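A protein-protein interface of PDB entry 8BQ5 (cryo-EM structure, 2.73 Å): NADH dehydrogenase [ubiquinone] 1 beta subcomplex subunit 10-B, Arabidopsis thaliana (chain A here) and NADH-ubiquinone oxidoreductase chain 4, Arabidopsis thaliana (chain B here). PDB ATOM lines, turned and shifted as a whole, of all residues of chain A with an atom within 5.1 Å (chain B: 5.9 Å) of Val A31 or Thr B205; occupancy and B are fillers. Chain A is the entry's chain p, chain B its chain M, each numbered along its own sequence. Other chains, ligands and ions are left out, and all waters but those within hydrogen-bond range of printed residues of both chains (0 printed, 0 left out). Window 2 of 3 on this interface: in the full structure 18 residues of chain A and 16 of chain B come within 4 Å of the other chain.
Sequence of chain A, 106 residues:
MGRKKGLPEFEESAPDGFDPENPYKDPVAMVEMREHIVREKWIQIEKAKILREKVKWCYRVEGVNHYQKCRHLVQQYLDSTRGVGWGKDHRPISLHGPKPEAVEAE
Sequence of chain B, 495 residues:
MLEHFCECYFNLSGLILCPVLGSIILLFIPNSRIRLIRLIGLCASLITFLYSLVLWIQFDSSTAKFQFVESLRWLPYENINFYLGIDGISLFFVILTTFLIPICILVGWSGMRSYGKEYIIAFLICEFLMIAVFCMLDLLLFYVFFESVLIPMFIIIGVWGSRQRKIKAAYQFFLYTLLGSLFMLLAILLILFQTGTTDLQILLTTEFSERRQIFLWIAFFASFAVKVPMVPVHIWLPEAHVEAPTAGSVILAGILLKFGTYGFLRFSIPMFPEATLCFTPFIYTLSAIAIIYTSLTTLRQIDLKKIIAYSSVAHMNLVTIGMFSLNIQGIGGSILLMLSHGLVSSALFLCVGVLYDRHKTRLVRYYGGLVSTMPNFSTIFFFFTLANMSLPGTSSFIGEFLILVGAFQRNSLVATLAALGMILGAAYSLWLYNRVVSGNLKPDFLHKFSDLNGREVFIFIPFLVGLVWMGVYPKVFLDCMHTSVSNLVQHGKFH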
ATOM      1  N   TYR A  24     -26.948   8.514 -12.121  1.00  0.00           N
ATOM      2  CA  TYR A  24     -27.477   7.338 -11.437  1.00  0.00           C
ATOM      3  C   TYR A  24     -28.934   7.074 -11.812  1.00  0.00           C
ATOM      4  O   TYR A  24     -29.781   6.831 -10.956  1.00  0.00           O
ATOM      5  CB  TYR A  24     -27.322   7.511  -9.932  1.00  0.00           C
ATOM      6  CG  TYR A  24     -25.889   7.432  -9.465  1.00  0.00           C
ATOM      7  CD1 TYR A  24     -25.079   8.560  -9.456  1.00  0.00           C
ATOM      8  CD2 TYR A  24     -25.342   6.229  -9.040  1.00  0.00           C
ATOM      9  CE1 TYR A  24     -23.765   8.493  -9.033  1.00  0.00           C
ATOM     10  CE2 TYR A  24     -24.031   6.152  -8.616  1.00  0.00           C
ATOM     11  CZ  TYR A  24     -23.248   7.286  -8.614  1.00  0.00           C
ATOM     12  OH  TYR A  24     -21.941   7.209  -8.191  1.00  0.00           O
ATOM     13  N   PRO A  27     -28.422   2.460 -14.979  1.00  0.00           N
ATOM     14  CA  PRO A  27     -27.300   1.724 -14.376  1.00  0.00           C
ATOM     15  C   PRO A  27     -26.320   1.154 -15.418  1.00  0.00           C
ATOM     16  O   PRO A  27     -25.142   1.351 -15.250  1.00  0.00           O
ATOM     17  CB  PRO A  27     -27.997   0.612 -13.574  1.00  0.00           C
ATOM     18  CG  PRO A  27     -29.366   0.475 -14.194  1.00  0.00           C
ATOM     19  CD  PRO A  27     -29.720   1.873 -14.648  1.00  0.00           C
ATOM     20  N   VAL A  28     -26.826   0.495 -16.462  1.00  0.00           N
ATOM     21  CA  VAL A  28     -25.964  -0.108 -17.523  1.00  0.00           C
ATOM     22  C   VAL A  28     -25.113   0.984 -18.194  1.00  0.00           C
ATOM     23  O   VAL A  28     -23.893   0.768 -18.314  1.00  0.00           O
ATOM     24  CB  VAL A  28     -26.829  -0.884 -18.535  1.00  0.00           C
ATOM     25  CG1 VAL A  28     -26.083  -1.228 -19.814  1.00  0.00           C
ATOM     26  CG2 VAL A  28     -27.428  -2.135 -17.912  1.00  0.00           C
ATOM     27  N   ALA A  29     -25.717   2.107 -18.603  1.00  0.00           N
ATOM     28  CA  ALA A  29     -24.973   3.171 -19.329  1.00  0.00           C
ATOM     29  C   ALA A  29     -23.931   3.823 -18.421  1.00  0.00           C
ATOM     30  O   ALA A  29     -22.828   4.049 -18.904  1.00  0.00           O
ATOM     31  CB  ALA A  29     -25.926   4.203 -19.871  1.00  0.00           C
ATOM     32  N   MET A  30     -24.279   4.118 -17.169  1.00  0.00           N
ATOM     33  CA  MET A  30     -23.315   4.698 -16.191  1.00  0.00           C
ATOM     34  C   MET A  30     -22.018   3.875 -16.170  1.00  0.00           C
ATOM     35  O   MET A  30     -20.942   4.490 -16.113  1.00  0.00           O
ATOM     36  CB  MET A  30     -23.927   4.697 -14.788  1.00  0.00           C
ATOM     37  CG  MET A  30     -23.180   5.573 -13.810  1.00  0.00           C
ATOM     38  SD  MET A  30     -22.995   4.866 -12.156  1.00  0.00           S
ATOM     39  CE  MET A  30     -21.438   3.999 -12.337  1.00  0.00           C
ATOM     40  N   VAL A  31     -22.120   2.542 -16.214  1.00  0.00           N
ATOM     41  CA  VAL A  31     -20.916   1.657 -16.178  1.00  0.00           C
ATOM     42  C   VAL A  31     -20.173   1.743 -17.517  1.00  0.00           C
ATOM     43  O   VAL A  31     -18.957   2.000 -17.492  1.00  0.00           O
ATOM     44  CB  VAL A  31     -21.281   0.208 -15.808  1.00  0.00           C
ATOM     45  CG1 VAL A  31     -20.069  -0.706 -15.784  1.00  0.00           C
ATOM     46  CG2 VAL A  31     -22.019   0.137 -14.484  1.00  0.00           C
ATOM     47  N   GLU A  32     -20.875   1.560 -18.642  1.00  0.00           N
ATOM     48  CA  GLU A  32     -20.218   1.652 -19.973  1.00  0.00           C
ATOM     49  C   GLU A  32     -19.654   3.063 -20.190  1.00  0.00           C
ATOM     50  O   GLU A  32     -18.676   3.180 -20.950  1.00  0.00           O
ATOM     51  CB  GLU A  32     -21.200   1.231 -21.068  1.00  0.00           C
ATOM     52  CG  GLU A  32     -20.585   1.228 -22.456  1.00  0.00           C
ATOM     53  CD  GLU A  32     -21.493   0.773 -23.588  1.00  0.00           C
ATOM     54  OE1 GLU A  32     -22.673   0.473 -23.322  1.00  0.00           O
ATOM     55  OE2 GLU A  32     -21.017   0.730 -24.738  1.00  0.00           O
ATOM     56  N   MET A  33     -20.237   4.092 -19.570  1.00  0.00           N
ATOM     57  CA  MET A  33     -19.688   5.442 -19.682  1.00  0.00           C
ATOM     58  C   MET A  33     -18.372   5.572 -18.925  1.00  0.00           C
ATOM     59  O   MET A  33     -17.425   6.197 -19.420  1.00  0.00           O
ATOM     60  CB  MET A  33     -20.702   6.465 -19.173  1.00  0.00           C
ATOM     61  CG  MET A  33     -20.233   7.914 -19.217  1.00  0.00           C
ATOM     62  SD  MET A  33     -19.994   8.598 -20.867  1.00  0.00           S
ATOM     63  CE  MET A  33     -19.433  10.246 -20.445  1.00  0.00           C
ATOM     64  N   ARG A  34     -18.295   4.998 -17.722  1.00  0.00           N
ATOM     65  CA  ARG A  34     -17.050   5.025 -16.960  1.00  0.00           C
ATOM     66  C   ARG A  34     -15.935   4.321 -17.719  1.00  0.00           C
ATOM     67  O   ARG A  34     -14.794   4.796 -17.760  1.00  0.00           O
ATOM     68  CB  ARG A  34     -17.262   4.378 -15.589  1.00  0.00           C
ATOM     69  CG  ARG A  34     -16.054   4.459 -14.668  1.00  0.00           C
ATOM     70  CD  ARG A  34     -16.201   3.535 -13.472  1.00  0.00           C
ATOM     71  NE  ARG A  34     -16.067   2.135 -13.847  1.00  0.00           N
ATOM     72  CZ  ARG A  34     -16.841   1.157 -13.399  1.00  0.00           C
ATOM     73  NH1 ARG A  34     -17.815   1.390 -12.535  1.00  0.00           N
ATOM     74  NH2 ARG A  34     -16.630  -0.085 -13.824  1.00  0.00           N
ATOM     75  N   GLU A  35     -16.263   3.184 -18.325  1.00  0.00           N
ATOM     76  CA  GLU A  35     -15.270   2.433 -19.131  1.00  0.00           C
ATOM     77  C   GLU A  35     -14.828   3.273 -20.327  1.00  0.00           C
ATOM     78  O   GLU A  35     -13.618   3.277 -20.616  1.00  0.00           O
ATOM     79  CB  GLU A  35     -15.901   1.139 -19.627  1.00  0.00           C
ATOM     80  CG  GLU A  35     -16.209   0.162 -18.516  1.00  0.00           C
ATOM     81  CD  GLU A  35     -16.903  -1.095 -19.008  1.00  0.00           C
ATOM     82  OE1 GLU A  35     -17.310  -1.119 -20.180  1.00  0.00           O
ATOM     83  OE2 GLU A  35     -17.011  -2.050 -18.218  1.00  0.00           O
ATOM     84  N   LYS B  65     -14.580  -5.520 -16.431  1.00  0.00           N
ATOM     85  CA  LYS B  65     -15.684  -6.358 -15.914  1.00  0.00           C
ATOM     86  C   LYS B  65     -15.073  -7.486 -15.082  1.00  0.00           C
ATOM     87  O   LYS B  65     -13.963  -7.947 -15.420  1.00  0.00           O
ATOM     88  CB  LYS B  65     -16.533  -6.868 -17.083  1.00  0.00           C
ATOM     89  CG  LYS B  65     -17.697  -5.974 -17.480  1.00  0.00           C
ATOM     90  CD  LYS B  65     -17.337  -4.954 -18.538  1.00  0.00           C
ATOM     91  CE  LYS B  65     -18.542  -4.213 -19.074  1.00  0.00           C
ATOM     92  NZ  LYS B  65     -19.634  -5.134 -19.466  1.00  0.00           N
ATOM     93  N   LEU B 200     -21.851  -6.556  -4.856  1.00  0.00           N
ATOM     94  CA  LEU B 200     -20.888  -5.505  -5.173  1.00  0.00           C
ATOM     95  C   LEU B 200     -21.205  -4.832  -6.499  1.00  0.00           C
ATOM     96  O   LEU B 200     -21.195  -3.600  -6.595  1.00  0.00           O
ATOM     97  CB  LEU B 200     -19.477  -6.085  -5.205  1.00  0.00           C
ATOM     98  CG  LEU B 200     -18.380  -5.105  -5.605  1.00  0.00           C
ATOM     99  CD1 LEU B 200     -18.199  -4.030  -4.543  1.00  0.00           C
ATOM    100  CD2 LEU B 200     -17.105  -5.866  -5.852  1.00  0.00           C
ATOM    101  N   GLN B 201     -21.490  -5.625  -7.535  1.00  0.00           N
ATOM    102  CA  GLN B 201     -21.763  -5.053  -8.849  1.00  0.00           C
ATOM    103  C   GLN B 201     -22.954  -4.108  -8.808  1.00  0.00           C
ATOM    104  O   GLN B 201     -23.034  -3.165  -9.604  1.00  0.00           O
ATOM    105  CB  GLN B 201     -22.003  -6.165  -9.866  1.00  0.00           C
ATOM    106  CG  GLN B 201     -20.747  -6.873 -10.313  1.00  0.00           C
ATOM    107  CD  GLN B 201     -21.004  -8.317 -10.672  1.00  0.00           C
ATOM    108  OE1 GLN B 201     -20.642  -8.773 -11.755  1.00  0.00           O
ATOM    109  NE2 GLN B 201     -21.624  -9.052  -9.756  1.00  0.00           N
ATOM    110  N   ILE B 202     -23.888  -4.338  -7.886  1.00  0.00           N
ATOM    111  CA  ILE B 202     -25.057  -3.473  -7.787  1.00  0.00           C
ATOM    112  C   ILE B 202     -24.725  -2.215  -6.993  1.00  0.00           C
ATOM    113  O   ILE B 202     -24.986  -1.095  -7.444  1.00  0.00           O
ATOM    114  CB  ILE B 202     -26.242  -4.238  -7.173  1.00  0.00           C
ATOM    115  CG1 ILE B 202     -26.662  -5.391  -8.085  1.00  0.00           C
ATOM    116  CG2 ILE B 202     -27.414  -3.300  -6.942  1.00  0.00           C
ATOM    117  CD1 ILE B 202     -26.775  -5.007  -9.542  1.00  0.00           C
ATOM    118  N   LEU B 203     -24.136  -2.377  -5.802  1.00  0.00           N
ATOM    119  CA  LEU B 203     -23.842  -1.212  -4.970  1.00  0.00           C
ATOM    120  C   LEU B 203     -22.837  -0.282  -5.633  1.00  0.00           C
ATOM    121  O   LEU B 203     -22.800   0.912  -5.317  1.00  0.00           O
ATOM    122  CB  LEU B 203     -23.333  -1.636  -3.592  1.00  0.00           C
ATOM    123  CG  LEU B 203     -23.937  -2.868  -2.922  1.00  0.00           C
ATOM    124  CD1 LEU B 203     -23.133  -3.239  -1.690  1.00  0.00           C
ATOM    125  CD2 LEU B 203     -25.385  -2.627  -2.561  1.00  0.00           C
ATOM    126  N   LEU B 204     -22.078  -0.797  -6.603  1.00  0.00           N
ATOM    127  CA  LEU B 204     -21.174   0.100  -7.371  1.00  0.00           C
ATOM    128  C   LEU B 204     -22.030   1.044  -8.226  1.00  0.00           C
ATOM    129  O   LEU B 204     -21.528   2.127  -8.579  1.00  0.00           O
ATOM    130  CB  LEU B 204     -20.246  -0.748  -8.245  1.00  0.00           C
ATOM    131  CG  LEU B 204     -18.982  -1.266  -7.560  1.00  0.00           C
ATOM    132  CD1 LEU B 204     -17.901  -1.584  -8.580  1.00  0.00           C
ATOM    133  CD2 LEU B 204     -18.465  -0.278  -6.525  1.00  0.00           C
ATOM    134  N   THR B 205     -23.276   0.653  -8.524  1.00  0.00           N
ATOM    135  CA  THR B 205     -24.176   1.459  -9.398  1.00  0.00           C
ATOM    136  C   THR B 205     -25.232   2.224  -8.589  1.00  0.00           C
ATOM    137  O   THR B 205     -26.038   2.932  -9.219  1.00  0.00           O
ATOM    138  CB  THR B 205     -24.868   0.588 -10.455  1.00  0.00           C
ATOM    139  OG1 THR B 205     -25.652  -0.455  -9.872  1.00  0.00           O
ATOM    140  CG2 THR B 205     -23.869  -0.043 -11.397  1.00  0.00           C
ATOM    141  N   THR B 206     -25.230   2.108  -7.259  1.00  0.00           N
ATOM    142  CA  THR B 206     -26.183   2.847  -6.445  1.00  0.00           C
ATOM    143  C   THR B 206     -25.504   4.041  -5.786  1.00  0.00           C
ATOM    144  O   THR B 206     -24.422   3.934  -5.207  1.00  0.00           O
ATOM    145  CB  THR B 206     -26.813   1.954  -5.372  1.00  0.00           C
ATOM    146  OG1 THR B 206     -25.891   1.770  -4.292  1.00  0.00           O
ATOM    147  CG2 THR B 206     -27.199   0.603  -5.947  1.00  0.00           C
ATOM    148  N   GLU B 207     -26.163   5.191  -5.885  1.00  0.00           N
ATOM    149  CA  GLU B 207     -25.687   6.431  -5.285  1.00  0.00           C
ATOM    150  C   GLU B 207     -26.060   6.449  -3.810  1.00  0.00           C
ATOM    151  O   GLU B 207     -27.195   6.123  -3.448  1.00  0.00           O
ATOM    152  CB  GLU B 207     -26.276   7.650  -5.993  1.00  0.00           C
ATOM    153  CG  GLU B 207     -25.760   8.971  -5.457  1.00  0.00           C
ATOM    154  CD  GLU B 207     -26.324  10.158  -6.209  1.00  0.00           C
ATOM    155  OE1 GLU B 207     -27.146   9.944  -7.122  1.00  0.00           O
ATOM    156  OE2 GLU B 207     -25.945  11.305  -5.887  1.00  0.00           O
ATOM    157  N   ASN B 487     -10.129   2.005 -13.735  1.00  0.00           N
ATOM    158  CA  ASN B 487     -11.560   2.097 -13.483  1.00  0.00           C
ATOM    159  C   ASN B 487     -11.856   2.321 -12.008  1.00  0.00           C
ATOM    160  O   ASN B 487     -12.909   2.869 -11.664  1.00  0.00           O
ATOM    161  CB  ASN B 487     -12.257   0.835 -13.982  1.00  0.00           C
ATOM    162  CG  ASN B 487     -12.766   0.981 -15.396  1.00  0.00           C
ATOM    163  OD1 ASN B 487     -12.033   0.756 -16.355  1.00  0.00           O
ATOM    164  ND2 ASN B 487     -14.025   1.361 -15.536  1.00  0.00           N
ATOM    165  N   HIS B 491     -13.885   5.791 -10.918  1.00  0.00           N
ATOM    166  CA  HIS B 491     -15.221   5.510 -10.327  1.00  0.00           C
ATOM    167  C   HIS B 491     -15.796   6.728  -9.606  1.00  0.00           C
ATOM    168  O   HIS B 491     -15.099   7.309  -8.761  1.00  0.00           O
ATOM    169  CB  HIS B 491     -15.143   4.307  -9.379  1.00  0.00           C
ATOM    170  CG  HIS B 491     -16.471   3.693  -9.090  1.00  0.00           C
ATOM    171  ND1 HIS B 491     -16.892   2.530  -9.696  1.00  0.00           N
ATOM    172  CD2 HIS B 491     -17.473   4.077  -8.272  1.00  0.00           C
ATOM    173  CE1 HIS B 491     -18.097   2.223  -9.264  1.00  0.00           C
ATOM    174  NE2 HIS B 491     -18.475   3.154  -8.387  1.00  0.00           N
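ND2 of Asn B487 lies close to NE of Arg A34 (2.8 Å). ND1 of His B491 is in hydrogen-bond range of NH1 of Arg A34.
OG1 of Thr B205 lies within hydrogen-bond range of O of Ile B202, at 2.6 Å. OG1 of Thr B206 sits at hydrogen-bond distance from O of Leu B203 (3.4 Å). A ring nitrogen (NE2) of His B491 lies within hydrogen-bond range of the backbone carbonyl oxygen (O) of Leu B204 (3.2 Å).
O of Thr B205 touches CD2 of Tyr A24, at 3.4 Å. Thr B206 touches Tyr A24. OE1 of Glu B207 touches CD1 of Tyr A24 (3.4 Å). CG2 of Val A31 touches CG2 of Thr B205, at 3.6 Å. OE2 of Glu A35 touches CE of Lys B65 (2.8 Å). Asn B487 touches Glu A35.
Of the printed residues of chain B, Tyr A24 touches Thr B205 (3.4 Å), Thr B206 (3.8 Å) and Glu B207 (3.4 Å). Val A31 touches just one residue of chain B: Thr B205 (3.6 Å). Thr B205 touches just these residues of chain A: Tyr A24 (3.4 Å) and Val A31 (3.6 Å). Printed residues of chain A within 4 Å of Thr B206: Tyr A24 (3.8 Å). Printed residues of chain A within 4 Å of Glu B207: Tyr A24 (3.4 Å). Printed residues of chain A within 4 Å of Asn B487: Arg A34 and Glu A35. Printed residues of chain A within 4 Å of His B491: Arg A34. The nearest residue of chain B that does not touch Val A31 is Lys B65 (5.0 Å). The nearest printed residue of chain A that does not touch Lys B65 is Val A31 (5.0 Å).
Hydrophobic or aromatic side chains of chain A within 4 Å of the printed part of chain B: Tyr A24 and Val A31. Of the 11 printed residues of chain B, 6 touch a printed residue of chain A. Among the printed residues, no Asp or Glu carboxylate lies within 4 Å of a Lys or Arg side-chain nitrogen of the other chain.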
